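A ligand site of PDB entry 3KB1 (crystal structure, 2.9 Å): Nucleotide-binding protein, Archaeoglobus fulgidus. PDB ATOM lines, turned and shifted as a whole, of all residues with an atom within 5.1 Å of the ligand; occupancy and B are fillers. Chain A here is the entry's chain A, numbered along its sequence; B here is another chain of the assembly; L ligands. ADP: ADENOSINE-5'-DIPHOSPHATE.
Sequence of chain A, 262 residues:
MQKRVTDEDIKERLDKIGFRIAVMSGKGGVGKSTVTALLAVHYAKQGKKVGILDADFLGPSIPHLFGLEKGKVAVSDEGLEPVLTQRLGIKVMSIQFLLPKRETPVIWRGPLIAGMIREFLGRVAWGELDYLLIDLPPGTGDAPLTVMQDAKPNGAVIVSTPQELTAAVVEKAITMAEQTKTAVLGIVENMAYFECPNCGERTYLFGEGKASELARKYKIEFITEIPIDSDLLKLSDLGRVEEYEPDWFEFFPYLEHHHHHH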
ATOM      1  N   SER A  25     -36.178 -31.092  -6.747  1.00  0.00           N
ATOM      2  CA  SER A  25     -35.065 -31.143  -5.794  1.00  0.00           C
ATOM      3  C   SER A  25     -35.499 -30.768  -4.387  1.00  0.00           C
ATOM      4  O   SER A  25     -36.449 -30.029  -4.212  1.00  0.00           O
ATOM      5  CB  SER A  25     -33.962 -30.182  -6.231  1.00  0.00           C
ATOM      6  OG  SER A  25     -34.429 -28.840  -6.194  1.00  0.00           O
ATOM      7  N   LYS A  27     -34.161 -28.823  -2.621  1.00  0.00           N
ATOM      8  CA  LYS A  27     -33.833 -27.407  -2.444  1.00  0.00           C
ATOM      9  C   LYS A  27     -32.987 -26.864  -3.610  1.00  0.00           C
ATOM     10  O   LYS A  27     -32.878 -27.507  -4.667  1.00  0.00           O
ATOM     11  CB  LYS A  27     -33.076 -27.189  -1.130  1.00  0.00           C
ATOM     12  CG  LYS A  27     -31.755 -27.926  -1.020  1.00  0.00           C
ATOM     13  CD  LYS A  27     -31.057 -27.612   0.300  1.00  0.00           C
ATOM     14  CE  LYS A  27     -30.464 -26.224   0.330  1.00  0.00           C
ATOM     15  NZ  LYS A  27     -29.848 -25.989   1.668  1.00  0.00           N
ATOM     16  N   GLY A  28     -32.410 -25.684  -3.429  1.00  0.00           N
ATOM     17  CA  GLY A  28     -31.590 -25.121  -4.487  1.00  0.00           C
ATOM     18  C   GLY A  28     -30.144 -25.521  -4.283  1.00  0.00           C
ATOM     19  O   GLY A  28     -29.818 -26.153  -3.273  1.00  0.00           O
ATOM     20  N   GLY A  29     -29.295 -25.174  -5.240  1.00  0.00           N
ATOM     21  CA  GLY A  29     -27.878 -25.488  -5.146  1.00  0.00           C
ATOM     22  C   GLY A  29     -27.547 -26.931  -5.473  1.00  0.00           C
ATOM     23  O   GLY A  29     -26.433 -27.227  -5.918  1.00  0.00           O
ATOM     24  N   VAL A  30     -28.512 -27.808  -5.265  1.00  0.00           N
ATOM     25  CA  VAL A  30     -28.393 -29.247  -5.527  1.00  0.00           C
ATOM     26  C   VAL A  30     -27.970 -29.509  -6.984  1.00  0.00           C
ATOM     27  O   VAL A  30     -27.389 -30.542  -7.293  1.00  0.00           O
ATOM     28  CB  VAL A  30     -29.752 -29.968  -5.204  1.00  0.00           C
ATOM     29  CG1 VAL A  30     -30.051 -29.969  -3.683  1.00  0.00           C
ATOM     30  CG2 VAL A  30     -30.882 -29.263  -5.916  1.00  0.00           C
ATOM     31  N   GLY A  31     -28.252 -28.548  -7.857  1.00  0.00           N
ATOM     32  CA  GLY A  31     -27.939 -28.670  -9.277  1.00  0.00           C
ATOM     33  C   GLY A  31     -29.077 -29.329 -10.052  1.00  0.00           C
ATOM     34  O   GLY A  31     -28.853 -30.305 -10.755  1.00  0.00           O
ATOM     35  N   LYS A  32     -30.295 -28.789  -9.928  1.00  0.00           N
ATOM     36  CA  LYS A  32     -31.481 -29.322 -10.616  1.00  0.00           C
ATOM     37  C   LYS A  32     -31.570 -28.947 -12.078  1.00  0.00           C
ATOM     38  O   LYS A  32     -31.909 -29.777 -12.934  1.00  0.00           O
ATOM     39  CB  LYS A  32     -32.763 -28.819  -9.936  1.00  0.00           C
ATOM     40  CG  LYS A  32     -34.056 -29.100 -10.751  1.00  0.00           C
ATOM     41  CD  LYS A  32     -35.270 -28.440 -10.102  1.00  0.00           C
ATOM     42  CE  LYS A  32     -34.917 -27.044  -9.686  1.00  0.00           C
ATOM     43  NZ  LYS A  32     -34.322 -26.344 -10.861  1.00  0.00           N
ATOM     44  N   SER A  33     -31.301 -27.673 -12.338  1.00  0.00           N
ATOM     45  CA  SER A  33     -31.335 -27.082 -13.672  1.00  0.00           C
ATOM     46  C   SER A  33     -30.183 -27.603 -14.525  1.00  0.00           C
ATOM     47  O   SER A  33     -30.364 -27.823 -15.719  1.00  0.00           O
ATOM     48  CB  SER A  33     -31.269 -25.563 -13.567  1.00  0.00           C
ATOM     49  OG  SER A  33     -32.365 -25.033 -12.825  1.00  0.00           O
ATOM     50  N   THR A  34     -29.007 -27.798 -13.927  1.00  0.00           N
ATOM     51  CA  THR A  34     -27.857 -28.316 -14.678  1.00  0.00           C
ATOM     52  C   THR A  34     -28.150 -29.737 -15.074  1.00  0.00           C
ATOM     53  O   THR A  34     -27.881 -30.141 -16.202  1.00  0.00           O
ATOM     54  CB  THR A  34     -26.555 -28.347 -13.856  1.00  0.00           C
ATOM     55  OG1 THR A  34     -26.071 -27.015 -13.659  1.00  0.00           O
ATOM     56  CG2 THR A  34     -25.486 -29.166 -14.604  1.00  0.00           C
ATOM     57  N   VAL A  35     -28.696 -30.510 -14.136  1.00  0.00           N
ATOM     58  CA  VAL A  35     -29.027 -31.882 -14.462  1.00  0.00           C
ATOM     59  C   VAL A  35     -30.067 -31.871 -15.582  1.00  0.00           C
ATOM     60  O   VAL A  35     -29.896 -32.574 -16.562  1.00  0.00           O
ATOM     61  CB  VAL A  35     -29.562 -32.666 -13.261  1.00  0.00           C
ATOM     62  CG1 VAL A  35     -30.311 -33.900 -13.764  1.00  0.00           C
ATOM     63  CG2 VAL A  35     -28.396 -33.105 -12.374  1.00  0.00           C
ATOM     64  N   ASP A  56     -38.575 -22.648 -13.225  1.00  0.00           N
ATOM     65  CA  ASP A  56     -37.879 -22.183 -12.026  1.00  0.00           C
ATOM     66  C   ASP A  56     -37.827 -20.660 -12.061  1.00  0.00           C
ATOM     67  O   ASP A  56     -36.852 -20.081 -12.534  1.00  0.00           O
ATOM     68  CB  ASP A  56     -36.462 -22.770 -11.972  1.00  0.00           C
ATOM     69  CG  ASP A  56     -35.793 -22.567 -10.624  1.00  0.00           C
ATOM     70  OD1 ASP A  56     -34.655 -23.070 -10.438  1.00  0.00           O
ATOM     71  OD2 ASP A  56     -36.392 -21.918  -9.751  1.00  0.00           O
ATOM     72  N   GLY A  59     -34.859 -18.909  -9.649  1.00  0.00           N
ATOM     73  CA  GLY A  59     -33.538 -18.750 -10.248  1.00  0.00           C
ATOM     74  C   GLY A  59     -33.395 -19.459 -11.580  1.00  0.00           C
ATOM     75  O   GLY A  59     -32.884 -20.592 -11.630  1.00  0.00           O
ATOM     76  N   SER A  61     -31.791 -20.674 -14.636  1.00  0.00           N
ATOM     77  CA  SER A  61     -30.447 -20.879 -15.112  1.00  0.00           C
ATOM     78  C   SER A  61     -30.427 -21.663 -16.399  1.00  0.00           C
ATOM     79  O   SER A  61     -29.372 -21.868 -17.000  1.00  0.00           O
ATOM     80  CB  SER A  61     -29.661 -21.618 -14.042  1.00  0.00           C
ATOM     81  OG  SER A  61     -30.544 -22.156 -13.073  1.00  0.00           O
ATOM     82  N   ASP A 135     -38.219 -28.104 -15.834  1.00  0.00           N
ATOM     83  CA  ASP A 135     -37.325 -27.766 -14.738  1.00  0.00           C
ATOM     84  C   ASP A 135     -38.160 -27.046 -13.658  1.00  0.00           C
ATOM     85  O   ASP A 135     -38.276 -25.819 -13.666  1.00  0.00           O
ATOM     86  CB  ASP A 135     -36.172 -26.874 -15.249  1.00  0.00           C
ATOM     87  CG  ASP A 135     -35.193 -26.460 -14.150  1.00  0.00           C
ATOM     88  OD1 ASP A 135     -35.019 -27.257 -13.198  1.00  0.00           O
ATOM     89  OD2 ASP A 135     -34.601 -25.358 -14.241  1.00  0.00           O
ATOM     90  N   PRO A 138     -37.122 -25.164  -7.157  1.00  0.00           N
ATOM     91  CA  PRO A 138     -36.521 -25.965  -6.101  1.00  0.00           C
ATOM     92  C   PRO A 138     -37.455 -26.242  -4.953  1.00  0.00           C
ATOM     93  O   PRO A 138     -38.438 -25.528  -4.744  1.00  0.00           O
ATOM     94  CB  PRO A 138     -35.328 -25.127  -5.668  1.00  0.00           C
ATOM     95  CG  PRO A 138     -35.821 -23.730  -5.867  1.00  0.00           C
ATOM     96  CD  PRO A 138     -36.488 -23.829  -7.228  1.00  0.00           C
ATOM     97  N   ASN A 190     -26.091 -35.490  -7.349  1.00  0.00           N
ATOM     98  CA  ASN A 190     -25.159 -34.522  -7.941  1.00  0.00           C
ATOM     99  C   ASN A 190     -23.991 -34.103  -7.046  1.00  0.00           C
ATOM    100  O   ASN A 190     -24.161 -33.911  -5.837  1.00  0.00           O
ATOM    101  CB  ASN A 190     -25.940 -33.284  -8.409  1.00  0.00           C
ATOM    102  CG  ASN A 190     -25.079 -32.301  -9.161  1.00  0.00           C
ATOM    103  OD1 ASN A 190     -23.995 -32.650  -9.645  1.00  0.00           O
ATOM    104  ND2 ASN A 190     -25.559 -31.062  -9.281  1.00  0.00           N
ATOM    105  N   MET A 191     -22.799 -33.945  -7.624  1.00  0.00           N
ATOM    106  CA  MET A 191     -21.617 -33.584  -6.837  1.00  0.00           C
ATOM    107  C   MET A 191     -21.462 -34.587  -5.693  1.00  0.00           C
ATOM    108  O   MET A 191     -21.605 -34.225  -4.527  1.00  0.00           O
ATOM    109  CB  MET A 191     -21.779 -32.180  -6.266  1.00  0.00           C
ATOM    110  CG  MET A 191     -21.977 -31.135  -7.339  1.00  0.00           C
ATOM    111  SD  MET A 191     -22.577 -29.374  -6.724  1.00  0.00           S
ATOM    112  CE  MET A 191     -20.841 -28.477  -6.750  1.00  0.00           C
ATOM    113  N   ILE A 226     -23.297 -38.037 -10.397  1.00  0.00           N
ATOM    114  CA  ILE A 226     -22.475 -37.099 -11.135  1.00  0.00           C
ATOM    115  C   ILE A 226     -21.496 -36.430 -10.182  1.00  0.00           C
ATOM    116  O   ILE A 226     -21.900 -35.736  -9.255  1.00  0.00           O
ATOM    117  CB  ILE A 226     -23.330 -36.033 -11.796  1.00  0.00           C
ATOM    118  CG1 ILE A 226     -24.446 -36.660 -12.613  1.00  0.00           C
ATOM    119  CG2 ILE A 226     -22.465 -35.186 -12.690  1.00  0.00           C
ATOM    120  CD1 ILE A 226     -25.338 -35.630 -13.280  1.00  0.00           C
ATOM    121  N   PRO A 227     -20.195 -36.599 -10.394  1.00  0.00           N
ATOM    122  CA  PRO A 227     -19.180 -35.991  -9.542  1.00  0.00           C
ATOM    123  C   PRO A 227     -19.055 -34.473  -9.792  1.00  0.00           C
ATOM    124  O   PRO A 227     -19.588 -33.971 -10.767  1.00  0.00           O
ATOM    125  CB  PRO A 227     -17.917 -36.721  -9.971  1.00  0.00           C
ATOM    126  CG  PRO A 227     -18.098 -36.832 -11.442  1.00  0.00           C
ATOM    127  CD  PRO A 227     -19.564 -37.277 -11.549  1.00  0.00           C
ATOM    128  N   ILE A 228     -18.356 -33.772  -8.892  1.00  0.00           N
ATOM    129  CA  ILE A 228     -18.113 -32.336  -9.015  1.00  0.00           C
ATOM    130  C   ILE A 228     -17.082 -32.224 -10.119  1.00  0.00           C
ATOM    131  O   ILE A 228     -15.890 -32.429  -9.880  1.00  0.00           O
ATOM    132  CB  ILE A 228     -17.505 -31.719  -7.720  1.00  0.00           C
ATOM    133  CG1 ILE A 228     -18.523 -31.709  -6.579  1.00  0.00           C
ATOM    134  CG2 ILE A 228     -16.997 -30.301  -8.019  1.00  0.00           C
ATOM    135  CD1 ILE A 228     -17.929 -31.363  -5.220  1.00  0.00           C
ATOM    136  N   ASP A 229     -17.547 -31.902 -11.321  1.00  0.00           N
ATOM    137  CA  ASP A 229     -16.690 -31.814 -12.500  1.00  0.00           C
ATOM    138  C   ASP A 229     -16.373 -30.372 -12.867  1.00  0.00           C
ATOM    139  O   ASP A 229     -17.227 -29.656 -13.380  1.00  0.00           O
ATOM    140  CB  ASP A 229     -17.377 -32.519 -13.676  1.00  0.00           C
ATOM    141  CG  ASP A 229     -16.540 -32.492 -14.937  1.00  0.00           C
ATOM    142  OD1 ASP A 229     -15.294 -32.416 -14.830  1.00  0.00           O
ATOM    143  OD2 ASP A 229     -17.147 -32.561 -16.042  1.00  0.00           O
ATOM    144  N   SER A 230     -15.137 -29.956 -12.623  1.00  0.00           N
ATOM    145  CA  SER A 230     -14.715 -28.579 -12.921  1.00  0.00           C
ATOM    146  C   SER A 230     -15.049 -28.180 -14.362  1.00  0.00           C
ATOM    147  O   SER A 230     -15.204 -26.997 -14.661  1.00  0.00           O
ATOM    148  CB  SER A 230     -13.216 -28.432 -12.677  1.00  0.00           C
ATOM    149  OG  SER A 230     -12.509 -29.381 -13.446  1.00  0.00           O
ATOM    150  N   LEU A 232     -17.789 -29.242 -16.205  1.00  0.00           N
ATOM    151  CA  LEU A 232     -19.223 -28.929 -16.316  1.00  0.00           C
ATOM    152  C   LEU A 232     -19.514 -27.550 -15.716  1.00  0.00           C
ATOM    153  O   LEU A 232     -20.543 -26.941 -15.994  1.00  0.00           O
ATOM    154  CB  LEU A 232     -20.068 -29.994 -15.592  1.00  0.00           C
ATOM    155  CG  LEU A 232     -21.591 -29.801 -15.656  1.00  0.00           C
ATOM    156  CD1 LEU A 232     -21.944 -29.438 -17.077  1.00  0.00           C
ATOM    157  CD2 LEU A 232     -22.352 -31.057 -15.214  1.00  0.00           C
ATOM    158  N   LEU A 233     -18.589 -27.051 -14.907  1.00  0.00           N
ATOM    159  CA  LEU A 233     -18.761 -25.758 -14.282  1.00  0.00           C
ATOM    160  C   LEU A 233     -18.231 -24.691 -15.207  1.00  0.00           C
ATOM    161  O   LEU A 233     -18.694 -23.554 -15.226  1.00  0.00           O
ATOM    162  CB  LEU A 233     -17.992 -25.712 -12.961  1.00  0.00           C
ATOM    163  CG  LEU A 233     -18.013 -24.400 -12.186  1.00  0.00           C
ATOM    164  CD1 LEU A 233     -19.442 -23.837 -12.108  1.00  0.00           C
ATOM    165  CD2 LEU A 233     -17.453 -24.683 -10.814  1.00  0.00           C
ATOM    166  N   SER A 236     -20.791 -24.521 -18.192  1.00  0.00           N
ATOM    167  CA  SER A 236     -22.093 -24.049 -17.745  1.00  0.00           C
ATOM    168  C   SER A 236     -22.084 -22.534 -17.732  1.00  0.00           C
ATOM    169  O   SER A 236     -23.057 -21.892 -18.129  1.00  0.00           O
ATOM    170  CB  SER A 236     -22.413 -24.560 -16.337  1.00  0.00           C
ATOM    171  OG  SER A 236     -22.897 -25.886 -16.381  1.00  0.00           O
ATOM    172  N   ASP A 237     -20.970 -21.953 -17.304  1.00  0.00           N
ATOM    173  CA  ASP A 237     -20.853 -20.515 -17.233  1.00  0.00           C
ATOM    174  C   ASP A 237     -20.702 -19.886 -18.595  1.00  0.00           C
ATOM    175  O   ASP A 237     -21.284 -18.837 -18.865  1.00  0.00           O
ATOM    176  CB  ASP A 237     -19.677 -20.136 -16.352  1.00  0.00           C
ATOM    177  CG  ASP A 237     -19.781 -20.770 -14.978  1.00  0.00           C
ATOM    178  OD1 ASP A 237     -19.023 -20.341 -14.066  1.00  0.00           O
ATOM    179  OD2 ASP A 237     -20.607 -21.699 -14.807  1.00  0.00           O
ATOM    180  N   GLN B 163     -16.763 -19.020  -8.654  1.00  0.00           N
ATOM    181  CA  GLN B 163     -17.610 -18.823  -9.813  1.00  0.00           C
ATOM    182  C   GLN B 163     -18.591 -17.687  -9.606  1.00  0.00           C
ATOM    183  O   GLN B 163     -19.373 -17.381 -10.493  1.00  0.00           O
ATOM    184  CB  GLN B 163     -18.368 -20.081 -10.113  1.00  0.00           C
ATOM    185  CG  GLN B 163     -19.390 -20.379  -9.094  1.00  0.00           C
ATOM    186  CD  GLN B 163     -20.268 -21.495  -9.537  1.00  0.00           C
ATOM    187  OE1 GLN B 163     -20.802 -21.458 -10.666  1.00  0.00           O
ATOM    188  NE2 GLN B 163     -20.441 -22.504  -8.685  1.00  0.00           N
HETATM  189  PB  ADP L   1     -30.473 -25.501  -8.970  1.00  0.00           P
HETATM  190  O1B ADP L   1     -31.229 -25.741 -10.215  1.00  0.00           O
HETATM  191  O2B ADP L   1     -31.012 -26.259  -7.808  1.00  0.00           O
HETATM  192  O3B ADP L   1     -30.696 -23.875  -8.557  1.00  0.00           O
HETATM  193  PA  ADP L   1     -28.017 -25.364 -10.274  1.00  0.00           P
HETATM  194  O1A ADP L   1     -27.967 -23.934 -10.680  1.00  0.00           O
HETATM  195  O2A ADP L   1     -28.217 -26.312 -11.373  1.00  0.00           O
HETATM  196  O3A ADP L   1     -28.982 -25.634  -9.130  1.00  0.00           O
HETATM  197  O5' ADP L   1     -26.518 -25.716  -9.729  1.00  0.00           O
HETATM  198  C5' ADP L   1     -25.830 -24.786  -8.883  1.00  0.00           C
HETATM  199  C4' ADP L   1     -24.343 -24.414  -9.210  1.00  0.00           C
HETATM  200  O4' ADP L   1     -23.577 -25.619  -9.083  1.00  0.00           O
HETATM  201  C3' ADP L   1     -24.021 -23.883 -10.667  1.00  0.00           C
HETATM  202  O3' ADP L   1     -22.860 -23.017 -10.704  1.00  0.00           O
HETATM  203  C2' ADP L   1     -23.772 -25.204 -11.358  1.00  0.00           C
HETATM  204  O2' ADP L   1     -23.177 -24.944 -12.645  1.00  0.00           O
HETATM  205  C1' ADP L   1     -22.860 -25.869 -10.313  1.00  0.00           C
HETATM  206  N9  ADP L   1     -22.801 -27.313 -10.443  1.00  0.00           N
HETATM  207  C8  ADP L   1     -23.851 -28.192 -10.466  1.00  0.00           C
HETATM  208  N7  ADP L   1     -23.499 -29.428 -10.568  1.00  0.00           N
HETATM  209  C5  ADP L   1     -22.112 -29.399 -10.619  1.00  0.00           C
HETATM  210  C6  ADP L   1     -21.117 -30.412 -10.729  1.00  0.00           C
HETATM  211  N6  ADP L   1     -21.390 -31.694 -10.814  1.00  0.00           N
HETATM  212  N1  ADP L   1     -19.808 -30.026 -10.742  1.00  0.00           N
HETATM  213  C2  ADP L   1     -19.497 -28.720 -10.661  1.00  0.00           C
HETATM  214  N3  ADP L   1     -20.344 -27.681 -10.553  1.00  0.00           N
HETATM  215  C4  ADP L   1     -21.658 -28.099 -10.531  1.00  0.00           C
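The side-chain amide oxygen of Gln 163 of chain B lies within hydrogen-bond range of an oxygen (O3') of the ligand, at 2.6 Å. The backbone NH (N) of Ser 33 sits at hydrogen-bond distance from an oxygen (O1B) of the ligand (2.9 Å). O1B of the ligand sits at hydrogen-bond distance from OG of Ser 33 (2.9 Å). The backbone carbonyl oxygen (O) of Pro 227 sits at hydrogen-bond distance from a nitrogen (N6) of the ligand (2.9 Å). The side-chain amide nitrogen of Asn 190 is in hydrogen-bond range of a nitrogen (N7) of the ligand, 2.9 Å away. The backbone NH (N) of Asp 229 is in hydrogen-bond range of a nitrogen (N1) of the ligand (3.0 Å). N of Thr 34 lies within hydrogen-bond range of O2A of the ligand, at 3.1 Å. O2A of the ligand lies within hydrogen-bond range of OG1 of Thr 34, 3.2 Å away. The backbone NH (N) of Gly 31 sits close to an oxygen (O3A) of the ligand (3.3 Å). N of Lys 32 lies within hydrogen-bond range of O1B of the ligand (3.2 Å). NZ of Lys 32 lies within salt-bridge range of O1B of the ligand (3.2 Å). The backbone NH of Gly 29 lies within hydrogen-bond range of an oxygen (O2B) of the ligand.
The side-chain amino group (NZ) of Lys 32 sits at hydrogen-bond distance from the side-chain hydroxyl (OG) of Ser 33 (3.1 Å). The side-chain hydroxyl (OG) of Ser 33 lies within hydrogen-bond range of the side-chain hydroxyl (OG) of Ser 61. ND2 of Asn 190 sits at hydrogen-bond distance from O of Val 30, 2.8 Å away. The side-chain amino group of Lys 32 is in salt-bridge range of the side-chain carboxylate of Asp 56 (3.3 Å). The backbone NH (N) of Met 191 is in hydrogen-bond range of the backbone carbonyl oxygen (O) of Ile 226. OG of Ser 236 lies within hydrogen-bond range of O of Leu 232 (2.6 Å). The side-chain hydroxyl (OG) of Ser 25 is in hydrogen-bond range of the backbone carbonyl oxygen (O) of Lys 27. The backbone carbonyl oxygen of Gly 59 is in hydrogen-bond range of the side-chain hydroxyl of Ser 61.
Lys 27 touches the ligand (O to O2B, 3.9 Å). CA of Gly 28 touches O2B of the ligand (3.6 Å). Val 30 touches the ligand. Ser 61 touches the ligand (OG to O1A, 3.9 Å). Met 191 touches the ligand (CG to N6, 3.6 Å). Ile 228 touches the ligand. Leu 233 touches the ligand (CD1 to O3', 3.8 Å). Ser 236 touches the ligand. Hydrophobic or aromatic side chains within 4 Å of the ligand: Val 30, Met 191, Ile 228 and Leu 233.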
